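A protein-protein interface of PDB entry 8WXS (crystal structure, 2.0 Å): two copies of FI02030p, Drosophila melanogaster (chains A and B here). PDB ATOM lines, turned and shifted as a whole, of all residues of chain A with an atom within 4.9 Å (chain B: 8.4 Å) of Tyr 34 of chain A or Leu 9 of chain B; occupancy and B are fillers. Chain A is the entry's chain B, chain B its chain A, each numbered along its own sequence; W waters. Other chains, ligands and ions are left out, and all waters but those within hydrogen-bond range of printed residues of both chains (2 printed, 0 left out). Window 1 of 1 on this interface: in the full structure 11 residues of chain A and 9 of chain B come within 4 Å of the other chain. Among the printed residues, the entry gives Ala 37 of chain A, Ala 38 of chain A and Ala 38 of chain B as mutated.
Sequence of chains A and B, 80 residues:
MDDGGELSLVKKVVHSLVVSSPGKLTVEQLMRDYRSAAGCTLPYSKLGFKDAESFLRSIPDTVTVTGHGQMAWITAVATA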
ATOM      1  N   GLU A   6     -34.324 -35.423  -8.272  1.00  0.00           N
ATOM      2  CA  GLU A   6     -32.912 -35.086  -8.138  1.00  0.00           C
ATOM      3  C   GLU A   6     -32.066 -35.792  -9.195  1.00  0.00           C
ATOM      4  O   GLU A   6     -31.150 -35.186  -9.764  1.00  0.00           O
ATOM      5  CB  GLU A   6     -32.431 -35.423  -6.725  1.00  0.00           C
ATOM      6  CG  GLU A   6     -30.928 -35.400  -6.547  1.00  0.00           C
ATOM      7  CD  GLU A   6     -30.522 -35.242  -5.095  1.00  0.00           C
ATOM      8  OE1 GLU A   6     -31.419 -35.146  -4.229  1.00  0.00           O
ATOM      9  OE2 GLU A   6     -29.304 -35.196  -4.818  1.00  0.00           O
ATOM     10  N   LEU A   9     -32.252 -33.879 -12.310  1.00  0.00           N
ATOM     11  CA  LEU A   9     -31.506 -32.627 -12.240  1.00  0.00           C
ATOM     12  C   LEU A   9     -30.003 -32.872 -12.282  1.00  0.00           C
ATOM     13  O   LEU A   9     -29.255 -32.075 -12.862  1.00  0.00           O
ATOM     14  CB  LEU A   9     -31.895 -31.861 -10.978  1.00  0.00           C
ATOM     15  CG  LEU A   9     -33.301 -31.264 -10.980  1.00  0.00           C
ATOM     16  CD1 LEU A   9     -33.593 -30.613  -9.644  1.00  0.00           C
ATOM     17  CD2 LEU A   9     -33.455 -30.254 -12.107  1.00  0.00           C
ATOM     18  N   VAL A  10     -29.538 -33.961 -11.666  1.00  0.00           N
ATOM     19  CA  VAL A  10     -28.118 -34.296 -11.731  1.00  0.00           C
ATOM     20  C   VAL A  10     -27.720 -34.637 -13.162  1.00  0.00           C
ATOM     21  O   VAL A  10     -26.634 -34.268 -13.628  1.00  0.00           O
ATOM     22  CB  VAL A  10     -27.798 -35.447 -10.759  1.00  0.00           C
ATOM     23  CG1 VAL A  10     -26.399 -35.995 -11.013  1.00  0.00           C
ATOM     24  CG2 VAL A  10     -27.942 -34.978  -9.317  1.00  0.00           C
ATOM     25  N   VAL A  13     -27.130 -31.488 -15.135  1.00  0.00           N
ATOM     26  CA  VAL A  13     -25.874 -30.821 -14.807  1.00  0.00           C
ATOM     27  C   VAL A  13     -24.704 -31.543 -15.461  1.00  0.00           C
ATOM     28  O   VAL A  13     -23.806 -30.909 -16.032  1.00  0.00           O
ATOM     29  CB  VAL A  13     -25.702 -30.721 -13.281  1.00  0.00           C
ATOM     30  CG1 VAL A  13     -24.299 -30.249 -12.938  1.00  0.00           C
ATOM     31  CG2 VAL A  13     -26.730 -29.773 -12.703  1.00  0.00           C
ATOM     32  N   VAL A  14     -24.694 -32.876 -15.389  1.00  0.00           N
ATOM     33  CA  VAL A  14     -23.642 -33.654 -16.037  1.00  0.00           C
ATOM     34  C   VAL A  14     -23.623 -33.373 -17.533  1.00  0.00           C
ATOM     35  O   VAL A  14     -22.559 -33.156 -18.129  1.00  0.00           O
ATOM     36  CB  VAL A  14     -23.831 -35.153 -15.740  1.00  0.00           C
ATOM     37  CG1 VAL A  14     -22.964 -36.009 -16.664  1.00  0.00           C
ATOM     38  CG2 VAL A  14     -23.523 -35.439 -14.278  1.00  0.00           C
ATOM     39  N   LEU A  17     -22.102 -30.004 -18.371  1.00  0.00           N
ATOM     40  CA  LEU A  17     -20.654 -29.971 -18.194  1.00  0.00           C
ATOM     41  C   LEU A  17     -19.936 -30.681 -19.336  1.00  0.00           C
ATOM     42  O   LEU A  17     -18.849 -30.260 -19.750  1.00  0.00           O
ATOM     43  CB  LEU A  17     -20.284 -30.593 -16.849  1.00  0.00           C
ATOM     44  CG  LEU A  17     -20.671 -29.786 -15.610  1.00  0.00           C
ATOM     45  CD1 LEU A  17     -20.458 -30.623 -14.372  1.00  0.00           C
ATOM     46  CD2 LEU A  17     -19.866 -28.494 -15.521  1.00  0.00           C
ATOM     47  N   LEU A  30     -14.344 -34.731 -15.628  1.00  0.00           N
ATOM     48  CA  LEU A  30     -15.747 -34.444 -15.338  1.00  0.00           C
ATOM     49  C   LEU A  30     -15.992 -34.376 -13.838  1.00  0.00           C
ATOM     50  O   LEU A  30     -16.732 -33.506 -13.359  1.00  0.00           O
ATOM     51  CB  LEU A  30     -16.643 -35.502 -15.979  1.00  0.00           C
ATOM     52  CG  LEU A  30     -18.123 -35.399 -15.610  1.00  0.00           C
ATOM     53  CD1 LEU A  30     -18.756 -34.183 -16.269  1.00  0.00           C
ATOM     54  CD2 LEU A  30     -18.861 -36.671 -15.987  1.00  0.00           C
ATOM     55  N   MET A  31     -15.372 -35.288 -13.085  1.00  0.00           N
ATOM     56  CA  MET A  31     -15.465 -35.281 -11.629  1.00  0.00           C
ATOM     57  C   MET A  31     -15.023 -33.933 -11.071  1.00  0.00           C
ATOM     58  O   MET A  31     -15.704 -33.329 -10.234  1.00  0.00           O
ATOM     59  CB  MET A  31     -14.582 -36.395 -11.056  1.00  0.00           C
ATOM     60  CG  MET A  31     -15.222 -37.773 -10.926  1.00  0.00           C
ATOM     61  SD  MET A  31     -16.979 -37.772 -10.565  1.00  0.00           S
ATOM     62  CE  MET A  31     -16.939 -38.240  -8.832  1.00  0.00           C
ATOM     63  N   ARG A  32     -13.867 -33.452 -11.532  1.00  0.00           N
ATOM     64  CA  ARG A  32     -13.331 -32.177 -11.069  1.00  0.00           C
ATOM     65  C   ARG A  32     -14.215 -31.018 -11.503  1.00  0.00           C
ATOM     66  O   ARG A  32     -14.386 -30.044 -10.760  1.00  0.00           O
ATOM     67  CB  ARG A  32     -11.914 -31.990 -11.608  1.00  0.00           C
ATOM     68  CG  ARG A  32     -10.855 -32.825 -10.912  1.00  0.00           C
ATOM     69  CD  ARG A  32      -9.468 -32.253 -11.168  1.00  0.00           C
ATOM     70  NE  ARG A  32      -9.083 -32.410 -12.566  1.00  0.00           N
ATOM     71  CZ  ARG A  32      -8.629 -33.537 -13.098  1.00  0.00           C
ATOM     72  NH1 ARG A  32      -8.466 -34.629 -12.369  1.00  0.00           N
ATOM     73  NH2 ARG A  32      -8.331 -33.570 -14.393  1.00  0.00           N
ATOM     74  N   ASP A  33     -14.770 -31.102 -12.713  1.00  0.00           N
ATOM     75  CA  ASP A  33     -15.636 -30.041 -13.213  1.00  0.00           C
ATOM     76  C   ASP A  33     -16.916 -29.949 -12.392  1.00  0.00           C
ATOM     77  O   ASP A  33     -17.367 -28.850 -12.049  1.00  0.00           O
ATOM     78  CB  ASP A  33     -15.956 -30.292 -14.686  1.00  0.00           C
ATOM     79  CG  ASP A  33     -14.787 -29.971 -15.599  1.00  0.00           C
ATOM     80  OD1 ASP A  33     -13.763 -29.458 -15.102  1.00  0.00           O
ATOM     81  OD2 ASP A  33     -14.887 -30.256 -16.812  1.00  0.00           O
ATOM     82  N   TYR A  34     -17.503 -31.097 -12.055  1.00  0.00           N
ATOM     83  CA  TYR A  34     -18.726 -31.097 -11.258  1.00  0.00           C
ATOM     84  C   TYR A  34     -18.467 -30.558  -9.859  1.00  0.00           C
ATOM     85  O   TYR A  34     -19.265 -29.772  -9.332  1.00  0.00           O
ATOM     86  CB  TYR A  34     -19.304 -32.512 -11.206  1.00  0.00           C
ATOM     87  CG  TYR A  34     -20.717 -32.596 -10.672  1.00  0.00           C
ATOM     88  CD1 TYR A  34     -20.987 -32.386  -9.328  1.00  0.00           C
ATOM     89  CD2 TYR A  34     -21.780 -32.890 -11.515  1.00  0.00           C
ATOM     90  CE1 TYR A  34     -22.269 -32.461  -8.836  1.00  0.00           C
ATOM     91  CE2 TYR A  34     -23.071 -32.973 -11.029  1.00  0.00           C
ATOM     92  CZ  TYR A  34     -23.306 -32.756  -9.687  1.00  0.00           C
ATOM     93  OH  TYR A  34     -24.581 -32.828  -9.186  1.00  0.00           O
ATOM     94  N   ARG A  35     -17.352 -30.966  -9.246  1.00  0.00           N
ATOM     95  CA  ARG A  35     -17.032 -30.535  -7.888  1.00  0.00           C
ATOM     96  C   ARG A  35     -16.855 -29.021  -7.819  1.00  0.00           C
ATOM     97  O   ARG A  35     -17.285 -28.380  -6.853  1.00  0.00           O
ATOM     98  CB  ARG A  35     -15.772 -31.264  -7.412  1.00  0.00           C
ATOM     99  CG  ARG A  35     -15.186 -30.838  -6.063  1.00  0.00           C
ATOM    100  CD  ARG A  35     -16.232 -30.641  -4.980  1.00  0.00           C
ATOM    101  NE  ARG A  35     -15.624 -30.176  -3.740  1.00  0.00           N
ATOM    102  CZ  ARG A  35     -15.459 -28.899  -3.423  1.00  0.00           C
ATOM    103  NH1 ARG A  35     -15.853 -27.929  -4.233  1.00  0.00           N
ATOM    104  NH2 ARG A  35     -14.883 -28.586  -2.266  1.00  0.00           N
ATOM    105  N   SER A  36     -16.238 -28.427  -8.840  1.00  0.00           N
ATOM    106  CA  SER A  36     -16.076 -26.976  -8.847  1.00  0.00           C
ATOM    107  C   SER A  36     -17.378 -26.265  -9.194  1.00  0.00           C
ATOM    108  O   SER A  36     -17.745 -25.284  -8.537  1.00  0.00           O
ATOM    109  CB  SER A  36     -14.975 -26.570  -9.826  1.00  0.00           C
ATOM    110  OG  SER A  36     -13.740 -27.171  -9.479  1.00  0.00           O
ATOM    111  N   ALA A  37     -18.089 -26.749 -10.216  1.00  0.00           N
ATOM    112  CA  ALA A  37     -19.287 -26.054 -10.677  1.00  0.00           C
ATOM    113  C   ALA A  37     -20.431 -26.164  -9.678  1.00  0.00           C
ATOM    114  O   ALA A  37     -21.230 -25.230  -9.550  1.00  0.00           O
ATOM    115  CB  ALA A  37     -19.720 -26.598 -12.038  1.00  0.00           C
ATOM    116  N   ALA A  38     -20.530 -27.285  -8.962  1.00  0.00           N
ATOM    117  CA  ALA A  38     -21.601 -27.467  -7.995  1.00  0.00           C
ATOM    118  C   ALA A  38     -21.169 -27.212  -6.559  1.00  0.00           C
ATOM    119  O   ALA A  38     -22.031 -27.020  -5.694  1.00  0.00           O
ATOM    120  CB  ALA A  38     -22.181 -28.882  -8.106  1.00  0.00           C
ATOM    121  N   GLY A  39     -19.867 -27.184  -6.284  1.00  0.00           N
ATOM    122  CA  GLY A  39     -19.400 -27.073  -4.919  1.00  0.00           C
ATOM    123  C   GLY A  39     -19.492 -28.352  -4.121  1.00  0.00           C
ATOM    124  O   GLY A  39     -19.355 -28.309  -2.894  1.00  0.00           O
ATOM    125  N   CYS A  40     -19.717 -29.487  -4.780  1.00  0.00           N
ATOM    126  CA  CYS A  40     -19.916 -30.758  -4.103  1.00  0.00           C
ATOM    127  C   CYS A  40     -19.653 -31.890  -5.087  1.00  0.00           C
ATOM    128  O   CYS A  40     -19.856 -31.741  -6.295  1.00  0.00           O
ATOM    129  CB  CYS A  40     -21.332 -30.867  -3.521  1.00  0.00           C
ATOM    130  SG  CYS A  40     -21.510 -32.070  -2.176  1.00  0.00           S
ATOM    131  N   THR A  41     -19.199 -33.019  -4.549  1.00  0.00           N
ATOM    132  CA  THR A  41     -18.822 -34.160  -5.376  1.00  0.00           C
ATOM    133  C   THR A  41     -20.025 -34.686  -6.149  1.00  0.00           C
ATOM    134  O   THR A  41     -21.154 -34.669  -5.654  1.00  0.00           O
ATOM    135  CB  THR A  41     -18.232 -35.263  -4.491  1.00  0.00           C
ATOM    136  OG1 THR A  41     -17.049 -34.773  -3.853  1.00  0.00           O
ATOM    137  CG2 THR A  41     -17.873 -36.507  -5.309  1.00  0.00           C
ATOM    138  N   LEU A  42     -19.776 -35.126  -7.391  1.00  0.00           N
ATOM    139  CA  LEU A  42     -20.749 -35.845  -8.204  1.00  0.00           C
ATOM    140  C   LEU A  42     -21.453 -36.872  -7.326  1.00  0.00           C
ATOM    141  O   LEU A  42     -20.802 -37.764  -6.771  1.00  0.00           O
ATOM    142  CB  LEU A  42     -20.047 -36.496  -9.401  1.00  0.00           C
ATOM    143  CG  LEU A  42     -20.749 -37.249 -10.541  1.00  0.00           C
ATOM    144  CD1 LEU A  42     -21.489 -38.496 -10.090  1.00  0.00           C
ATOM    145  CD2 LEU A  42     -21.691 -36.324 -11.282  1.00  0.00           C
ATOM    146  N   PRO A  43     -22.776 -36.773  -7.160  1.00  0.00           N
ATOM    147  CA  PRO A  43     -23.487 -37.527  -6.116  1.00  0.00           C
ATOM    148  C   PRO A  43     -23.843 -38.967  -6.490  1.00  0.00           C
ATOM    149  O   PRO A  43     -24.973 -39.419  -6.290  1.00  0.00           O
ATOM    150  CB  PRO A  43     -24.738 -36.675  -5.890  1.00  0.00           C
ATOM    151  CG  PRO A  43     -25.040 -36.133  -7.260  1.00  0.00           C
ATOM    152  CD  PRO A  43     -23.684 -35.874  -7.901  1.00  0.00           C
ATOM    153  N   ASP B   3     -27.413 -22.448 -13.938  1.00  0.00           N
ATOM    154  CA  ASP B   3     -27.180 -22.059 -15.329  1.00  0.00           C
ATOM    155  C   ASP B   3     -27.038 -23.288 -16.191  1.00  0.00           C
ATOM    156  O   ASP B   3     -27.739 -23.442 -17.182  1.00  0.00           O
ATOM    157  CB  ASP B   3     -25.942 -21.182 -15.450  1.00  0.00           C
ATOM    158  CG  ASP B   3     -26.290 -19.771 -15.843  1.00  0.00           C
ATOM    159  OD1 ASP B   3     -25.383 -18.917 -15.887  1.00  0.00           O
ATOM    160  OD2 ASP B   3     -27.498 -19.524 -16.088  1.00  0.00           O
ATOM    161  N   GLY B   4     -26.111 -24.153 -15.805  1.00  0.00           N
ATOM    162  CA  GLY B   4     -26.100 -25.511 -16.298  1.00  0.00           C
ATOM    163  C   GLY B   4     -27.073 -26.425 -15.585  1.00  0.00           C
ATOM    164  O   GLY B   4     -27.115 -27.623 -15.883  1.00  0.00           O
ATOM    165  N   GLY B   5     -27.855 -25.894 -14.643  1.00  0.00           N
ATOM    166  CA  GLY B   5     -28.744 -26.680 -13.807  1.00  0.00           C
ATOM    167  C   GLY B   5     -28.331 -26.780 -12.352  1.00  0.00           C
ATOM    168  O   GLY B   5     -29.032 -27.442 -11.579  1.00  0.00           O
ATOM    169  N   GLU B   6     -27.218 -26.154 -11.948  1.00  0.00           N
ATOM    170  CA  GLU B   6     -26.744 -26.293 -10.571  1.00  0.00           C
ATOM    171  C   GLU B   6     -27.683 -25.616  -9.577  1.00  0.00           C
ATOM    172  O   GLU B   6     -27.966 -26.168  -8.509  1.00  0.00           O
ATOM    173  CB  GLU B   6     -25.324 -25.739 -10.438  1.00  0.00           C
ATOM    174  CG  GLU B   6     -24.261 -26.554 -11.165  1.00  0.00           C
ATOM    175  CD  GLU B   6     -24.078 -26.157 -12.612  1.00  0.00           C
ATOM    176  OE1 GLU B   6     -24.900 -25.366 -13.113  1.00  0.00           O
ATOM    177  OE2 GLU B   6     -23.102 -26.621 -13.243  1.00  0.00           O
ATOM    178  N   LEU B   7     -28.172 -24.417  -9.900  1.00  0.00           N
ATOM    179  CA  LEU B   7     -29.057 -23.720  -8.970  1.00  0.00           C
ATOM    180  C   LEU B   7     -30.365 -24.477  -8.779  1.00  0.00           C
ATOM    181  O   LEU B   7     -30.858 -24.609  -7.653  1.00  0.00           O
ATOM    182  CB  LEU B   7     -29.338 -22.298  -9.454  1.00  0.00           C
ATOM    183  CG  LEU B   7     -30.269 -21.507  -8.528  1.00  0.00           C
ATOM    184  CD1 LEU B   7     -29.693 -21.443  -7.120  1.00  0.00           C
ATOM    185  CD2 LEU B   7     -30.548 -20.107  -9.062  1.00  0.00           C
ATOM    186  N   SER B   8     -30.954 -24.969  -9.877  1.00  0.00           N
ATOM    187  CA  SER B   8     -32.201 -25.721  -9.777  1.00  0.00           C
ATOM    188  C   SER B   8     -32.037 -26.952  -8.902  1.00  0.00           C
ATOM    189  O   SER B   8     -32.989 -27.379  -8.238  1.00  0.00           O
ATOM    190  CB  SER B   8     -32.688 -26.131 -11.167  1.00  0.00           C
ATOM    191  OG  SER B   8     -33.021 -25.000 -11.950  1.00  0.00           O
ATOM    192  N   LEU B   9     -30.838 -27.532  -8.886  1.00  0.00           N
ATOM    193  CA  LEU B   9     -30.600 -28.698  -8.046  1.00  0.00           C
ATOM    194  C   LEU B   9     -30.502 -28.305  -6.576  1.00  0.00           C
ATOM    195  O   LEU B   9     -30.998 -29.027  -5.702  1.00  0.00           O
ATOM    196  CB  LEU B   9     -29.341 -29.418  -8.521  1.00  0.00           C
ATOM    197  CG  LEU B   9     -28.819 -30.570  -7.674  1.00  0.00           C
ATOM    198  CD1 LEU B   9     -29.748 -31.758  -7.793  1.00  0.00           C
ATOM    199  CD2 LEU B   9     -27.432 -30.936  -8.157  1.00  0.00           C
ATOM    200  N   VAL B  10     -29.879 -27.158  -6.283  1.00  0.00           N
ATOM    201  CA  VAL B  10     -29.841 -26.668  -4.907  1.00  0.00           C
ATOM    202  C   VAL B  10     -31.243 -26.315  -4.426  1.00  0.00           C
ATOM    203  O   VAL B  10     -31.607 -26.588  -3.275  1.00  0.00           O
ATOM    204  CB  VAL B  10     -28.885 -25.466  -4.788  1.00  0.00           C
ATOM    205  CG1 VAL B  10     -28.949 -24.873  -3.390  1.00  0.00           C
ATOM    206  CG2 VAL B  10     -27.464 -25.883  -5.117  1.00  0.00           C
ATOM    207  N   LYS B  11     -32.047 -25.698  -5.296  1.00  0.00           N
ATOM    208  CA  LYS B  11     -33.416 -25.346  -4.930  1.00  0.00           C
ATOM    209  C   LYS B  11     -34.216 -26.585  -4.560  1.00  0.00           C
ATOM    210  O   LYS B  11     -34.946 -26.596  -3.562  1.00  0.00           O
ATOM    211  CB  LYS B  11     -34.097 -24.616  -6.086  1.00  0.00           C
ATOM    212  CG  LYS B  11     -33.628 -23.202  -6.334  1.00  0.00           C
ATOM    213  CD  LYS B  11     -34.322 -22.649  -7.574  1.00  0.00           C
ATOM    214  CE  LYS B  11     -33.969 -21.197  -7.828  1.00  0.00           C
ATOM    215  NZ  LYS B  11     -34.638 -20.678  -9.059  1.00  0.00           N
ATOM    216  N   LYS B  12     -34.095 -27.643  -5.362  1.00  0.00           N
ATOM    217  CA  LYS B  12     -34.899 -28.828  -5.109  1.00  0.00           C
ATOM    218  C   LYS B  12     -34.499 -29.476  -3.788  1.00  0.00           C
ATOM    219  O   LYS B  12     -35.362 -29.919  -3.022  1.00  0.00           O
ATOM    220  CB  LYS B  12     -34.772 -29.806  -6.280  1.00  0.00           C
ATOM    221  CG  LYS B  12     -34.719 -31.276  -5.898  1.00  0.00           C
ATOM    222  CD  LYS B  12     -36.120 -31.791  -5.579  1.00  0.00           C
ATOM    223  CE  LYS B  12     -37.080 -31.534  -6.734  1.00  0.00           C
ATOM    224  NZ  LYS B  12     -38.417 -32.168  -6.537  1.00  0.00           N
ATOM    225  N   VAL B  13     -33.199 -29.504  -3.485  1.00  0.00           N
ATOM    226  CA  VAL B  13     -32.751 -30.050  -2.207  1.00  0.00           C
ATOM    227  C   VAL B  13     -33.269 -29.196  -1.058  1.00  0.00           C
ATOM    228  O   VAL B  13     -33.771 -29.712  -0.053  1.00  0.00           O
ATOM    229  CB  VAL B  13     -31.218 -30.164  -2.174  1.00  0.00           C
ATOM    230  CG1 VAL B  13     -30.752 -30.532  -0.775  1.00  0.00           C
ATOM    231  CG2 VAL B  13     -30.741 -31.195  -3.179  1.00  0.00           C
ATOM    232  N   VAL B  14     -33.155 -27.873  -1.194  1.00  0.00           N
ATOM    233  CA  VAL B  14     -33.603 -26.966  -0.141  1.00  0.00           C
ATOM    234  C   VAL B  14     -35.105 -27.093   0.069  1.00  0.00           C
ATOM    235  O   VAL B  14     -35.591 -27.166   1.204  1.00  0.00           O
ATOM    236  CB  VAL B  14     -33.206 -25.518  -0.479  1.00  0.00           C
ATOM    237  CG1 VAL B  14     -33.979 -24.531   0.389  1.00  0.00           C
ATOM    238  CG2 VAL B  14     -31.713 -25.330  -0.297  1.00  0.00           C
ATOM    239  N   HIS B  15     -35.866 -27.112  -1.025  1.00  0.00           N
ATOM    240  CA  HIS B  15     -37.314 -27.163  -0.877  1.00  0.00           C
ATOM    241  C   HIS B  15     -37.744 -28.471  -0.230  1.00  0.00           C
ATOM    242  O   HIS B  15     -38.669 -28.490   0.587  1.00  0.00           O
ATOM    243  CB  HIS B  15     -37.997 -26.976  -2.230  1.00  0.00           C
ATOM    244  CG  HIS B  15     -39.482 -27.163  -2.187  1.00  0.00           C
ATOM    245  ND1 HIS B  15     -40.080 -28.404  -2.170  1.00  0.00           N
ATOM    246  CD2 HIS B  15     -40.489 -26.259  -2.134  1.00  0.00           C
ATOM    247  CE1 HIS B  15     -41.393 -28.257  -2.121  1.00  0.00           C
ATOM    248  NE2 HIS B  15     -41.666 -26.965  -2.096  1.00  0.00           N
ATOM    249  N   SER B  16     -37.072 -29.573  -0.573  1.00  0.00           N
ATOM    250  CA  SER B  16     -37.387 -30.853   0.053  1.00  0.00           C
ATOM    251  C   SER B  16     -37.117 -30.810   1.549  1.00  0.00           C
ATOM    252  O   SER B  16     -37.887 -31.358   2.345  1.00  0.00           O
ATOM    253  CB  SER B  16     -36.579 -31.972  -0.604  1.00  0.00           C
ATOM    254  OG  SER B  16     -37.057 -32.247  -1.910  1.00  0.00           O
ATOM    255  N   TYR B  34     -29.084 -29.449   5.406  1.00  0.00           N
ATOM    256  CA  TYR B  34     -28.482 -29.517   4.076  1.00  0.00           C
ATOM    257  C   TYR B  34     -27.140 -30.239   4.126  1.00  0.00           C
ATOM    258  O   TYR B  34     -26.854 -31.105   3.292  1.00  0.00           O
ATOM    259  CB  TYR B  34     -28.318 -28.106   3.505  1.00  0.00           C
ATOM    260  CG  TYR B  34     -27.916 -28.050   2.043  1.00  0.00           C
ATOM    261  CD1 TYR B  34     -26.587 -28.175   1.658  1.00  0.00           C
ATOM    262  CD2 TYR B  34     -28.868 -27.852   1.051  1.00  0.00           C
ATOM    263  CE1 TYR B  34     -26.220 -28.119   0.318  1.00  0.00           C
ATOM    264  CE2 TYR B  34     -28.512 -27.789  -0.284  1.00  0.00           C
ATOM    265  CZ  TYR B  34     -27.188 -27.925  -0.645  1.00  0.00           C
ATOM    266  OH  TYR B  34     -26.833 -27.868  -1.971  1.00  0.00           O
ATOM    267  N   ALA B  38     -26.731 -33.480   1.869  1.00  0.00           N
ATOM    268  CA  ALA B  38     -25.860 -33.413   0.704  1.00  0.00           C
ATOM    269  C   ALA B  38     -24.395 -33.696   1.015  1.00  0.00           C
ATOM    270  O   ALA B  38     -23.615 -33.922   0.084  1.00  0.00           O
ATOM    271  CB  ALA B  38     -25.977 -32.036   0.039  1.00  0.00           C
ATOM    272  N   PRO B  43     -24.254 -23.892  -0.587  1.00  0.00           N
ATOM    273  CA  PRO B  43     -23.274 -23.171  -1.410  1.00  0.00           C
ATOM    274  C   PRO B  43     -23.565 -21.687  -1.643  1.00  0.00           C
ATOM    275  O   PRO B  43     -23.411 -21.173  -2.751  1.00  0.00           O
ATOM    276  CB  PRO B  43     -23.311 -23.958  -2.724  1.00  0.00           C
ATOM    277  CG  PRO B  43     -24.761 -24.338  -2.829  1.00  0.00           C
ATOM    278  CD  PRO B  43     -25.084 -24.795  -1.408  1.00  0.00           C
ATOM    279  N   LYS B  46     -20.204 -19.892  -2.755  1.00  0.00           N
ATOM    280  CA  LYS B  46     -19.817 -20.126  -4.143  1.00  0.00           C
ATOM    281  C   LYS B  46     -20.726 -19.375  -5.109  1.00  0.00           C
ATOM    282  O   LYS B  46     -20.277 -18.944  -6.179  1.00  0.00           O
ATOM    283  CB  LYS B  46     -19.813 -21.633  -4.428  1.00  0.00           C
ATOM    284  CG  LYS B  46     -20.016 -22.038  -5.880  1.00  0.00           C
ATOM    285  CD  LYS B  46     -20.617 -23.436  -5.968  1.00  0.00           C
ATOM    286  CE  LYS B  46     -22.066 -23.408  -6.436  1.00  0.00           C
ATOM    287  NZ  LYS B  46     -22.218 -23.094  -7.887  1.00  0.00           N
ATOM    288  N   PHE B  55     -28.468 -15.518   0.174  1.00  0.00           N
ATOM    289  CA  PHE B  55     -28.761 -16.506  -0.856  1.00  0.00           C
ATOM    290  C   PHE B  55     -30.230 -16.918  -0.819  1.00  0.00           C
ATOM    291  O   PHE B  55     -30.907 -16.936  -1.853  1.00  0.00           O
ATOM    292  CB  PHE B  55     -27.868 -17.736  -0.711  1.00  0.00           C
ATOM    293  CG  PHE B  55     -28.348 -18.899  -1.520  1.00  0.00           C
ATOM    294  CD1 PHE B  55     -28.418 -18.810  -2.901  1.00  0.00           C
ATOM    295  CD2 PHE B  55     -28.787 -20.057  -0.905  1.00  0.00           C
ATOM    296  CE1 PHE B  55     -28.892 -19.866  -3.657  1.00  0.00           C
ATOM    297  CE2 PHE B  55     -29.260 -21.118  -1.654  1.00  0.00           C
ATOM    298  CZ  PHE B  55     -29.309 -21.023  -3.030  1.00  0.00           C
HETATM  299  O   HOH W   1     -30.380 -29.393 -13.041  1.00  0.00           O
HETATM  300  O   HOH W   2     -24.665 -34.031  -2.480  1.00  0.00           O
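The side-chain amino group of Lys 46 of chain B is in hydrogen-bond range of the backbone carbonyl oxygen of Ala 37 of chain A (2.9 Å).
The backbone carbonyl oxygen (O) of Ala 38 of chain B lies close to the side-chain sulfur (SG) of Cys 40 of chain A.
OE1 of Glu 6 of chain B lies within hydrogen-bond range of N of Gly 4 of chain B.
The backbone carbonyl oxygen of Lys 12 of chain B lies within hydrogen-bond range of the side-chain hydroxyl of Ser 16 of chain B, 3.1 Å away.
O of Arg 35 of chain A is in hydrogen-bond range of N of Cys 40 of chain A (3.4 Å).
Among the printed residues, pairs that only touch across the chains: Leu 9 of chain A with Ser 8 of chain B (3.6 Å), Leu 9 of chain A with Leu 9 of chain B (3.8 Å), Leu 9 of chain A with Lys 12 of chain B (3.7 Å), Val 10 of chain A with Leu 9 of chain B (3.99 Å), Val 13 of chain A with Gly 4 of chain B (3.6 Å), Val 13 of chain A with Gly 5 of chain B (3.4 Å), Val 13 of chain A with Glu 6 of chain B (3.7 Å), Tyr 34 of chain A with Leu 9 of chain B (3.6 Å), Ala 37 of chain A with Glu 6 of chain B (3.6 Å), Ala 38 of chain A with Lys 46 of chain B (3.7 Å) and Gly 39 of chain A with Lys 46 of chain B (3.8 Å).
Of chain B, only Leu 9 (3.6 Å) comes within 4 Å of Tyr 34 of chain A.
Of the printed residues of chain A, Leu 9 of chain B touches Leu 9 (3.8 Å), Val 10 (3.99 Å) and Tyr 34 (3.6 Å).
Of the printed residues of chain B, Cys 40 of chain A touches Ala 38.
Printed residues of chain A within 4 Å of Lys 12 of chain B: Leu 9.
Of the printed residues of chain B, Ala 37 of chain A touches Glu 6 and Lys 46.
Tyr 34 of chain B touches none of the printed residues of chain A.
The nearest printed residue of chain A that does not touch Leu 9 of chain B is Glu 6 of chain A (4.03 Å).
The nearest printed residue of chain A that does not touch Ser 8 of chain B is Val 13 of chain A (7.0 Å).
Of the 20 printed residues of chain A, 8 touch a printed residue of chain B.
Of the 19 printed residues of chain B, 8 touch a printed residue of chain A.
Hydrophobic or aromatic side chains of chain B within 4 Å of the printed part of chain A: Leu 9.
Among the printed residues, no Asp or Glu carboxylate lies within 4 Å of a Lys or Arg side-chain nitrogen of the other chain.
Leu 9 of chain B touches its own counterpart, Leu 9 of chain A.
Val 10 of chain A touches Leu 9 of chain B, but with the chains exchanged Leu 9 of chain A does not touch Val 10 of chain B (6.1 Å).
Val 13 of chain A touches Glu 6 of chain B, but with the chains exchanged Glu 6 of chain A does not touch Val 13 of chain B (4.1 Å).
Tyr 34 of chain A touches Leu 9 of chain B, but with the chains exchanged Leu 9 of chain A does not touch Tyr 34 of chain B (10.6 Å).
Of the 13 pairs that touch across the chains among the printed residues, 1 has its exchanged pair printed and touching as well.
Water W2 bridges O of Ala 38 of chain B (2.8 Å) and SG of Cys 40 of chain A (3.7 Å).
Water W1 lies within hydrogen-bond range of O of Gly 5 of chain B (2.8 Å) and O of Leu 9 of chain A (2.9 Å).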
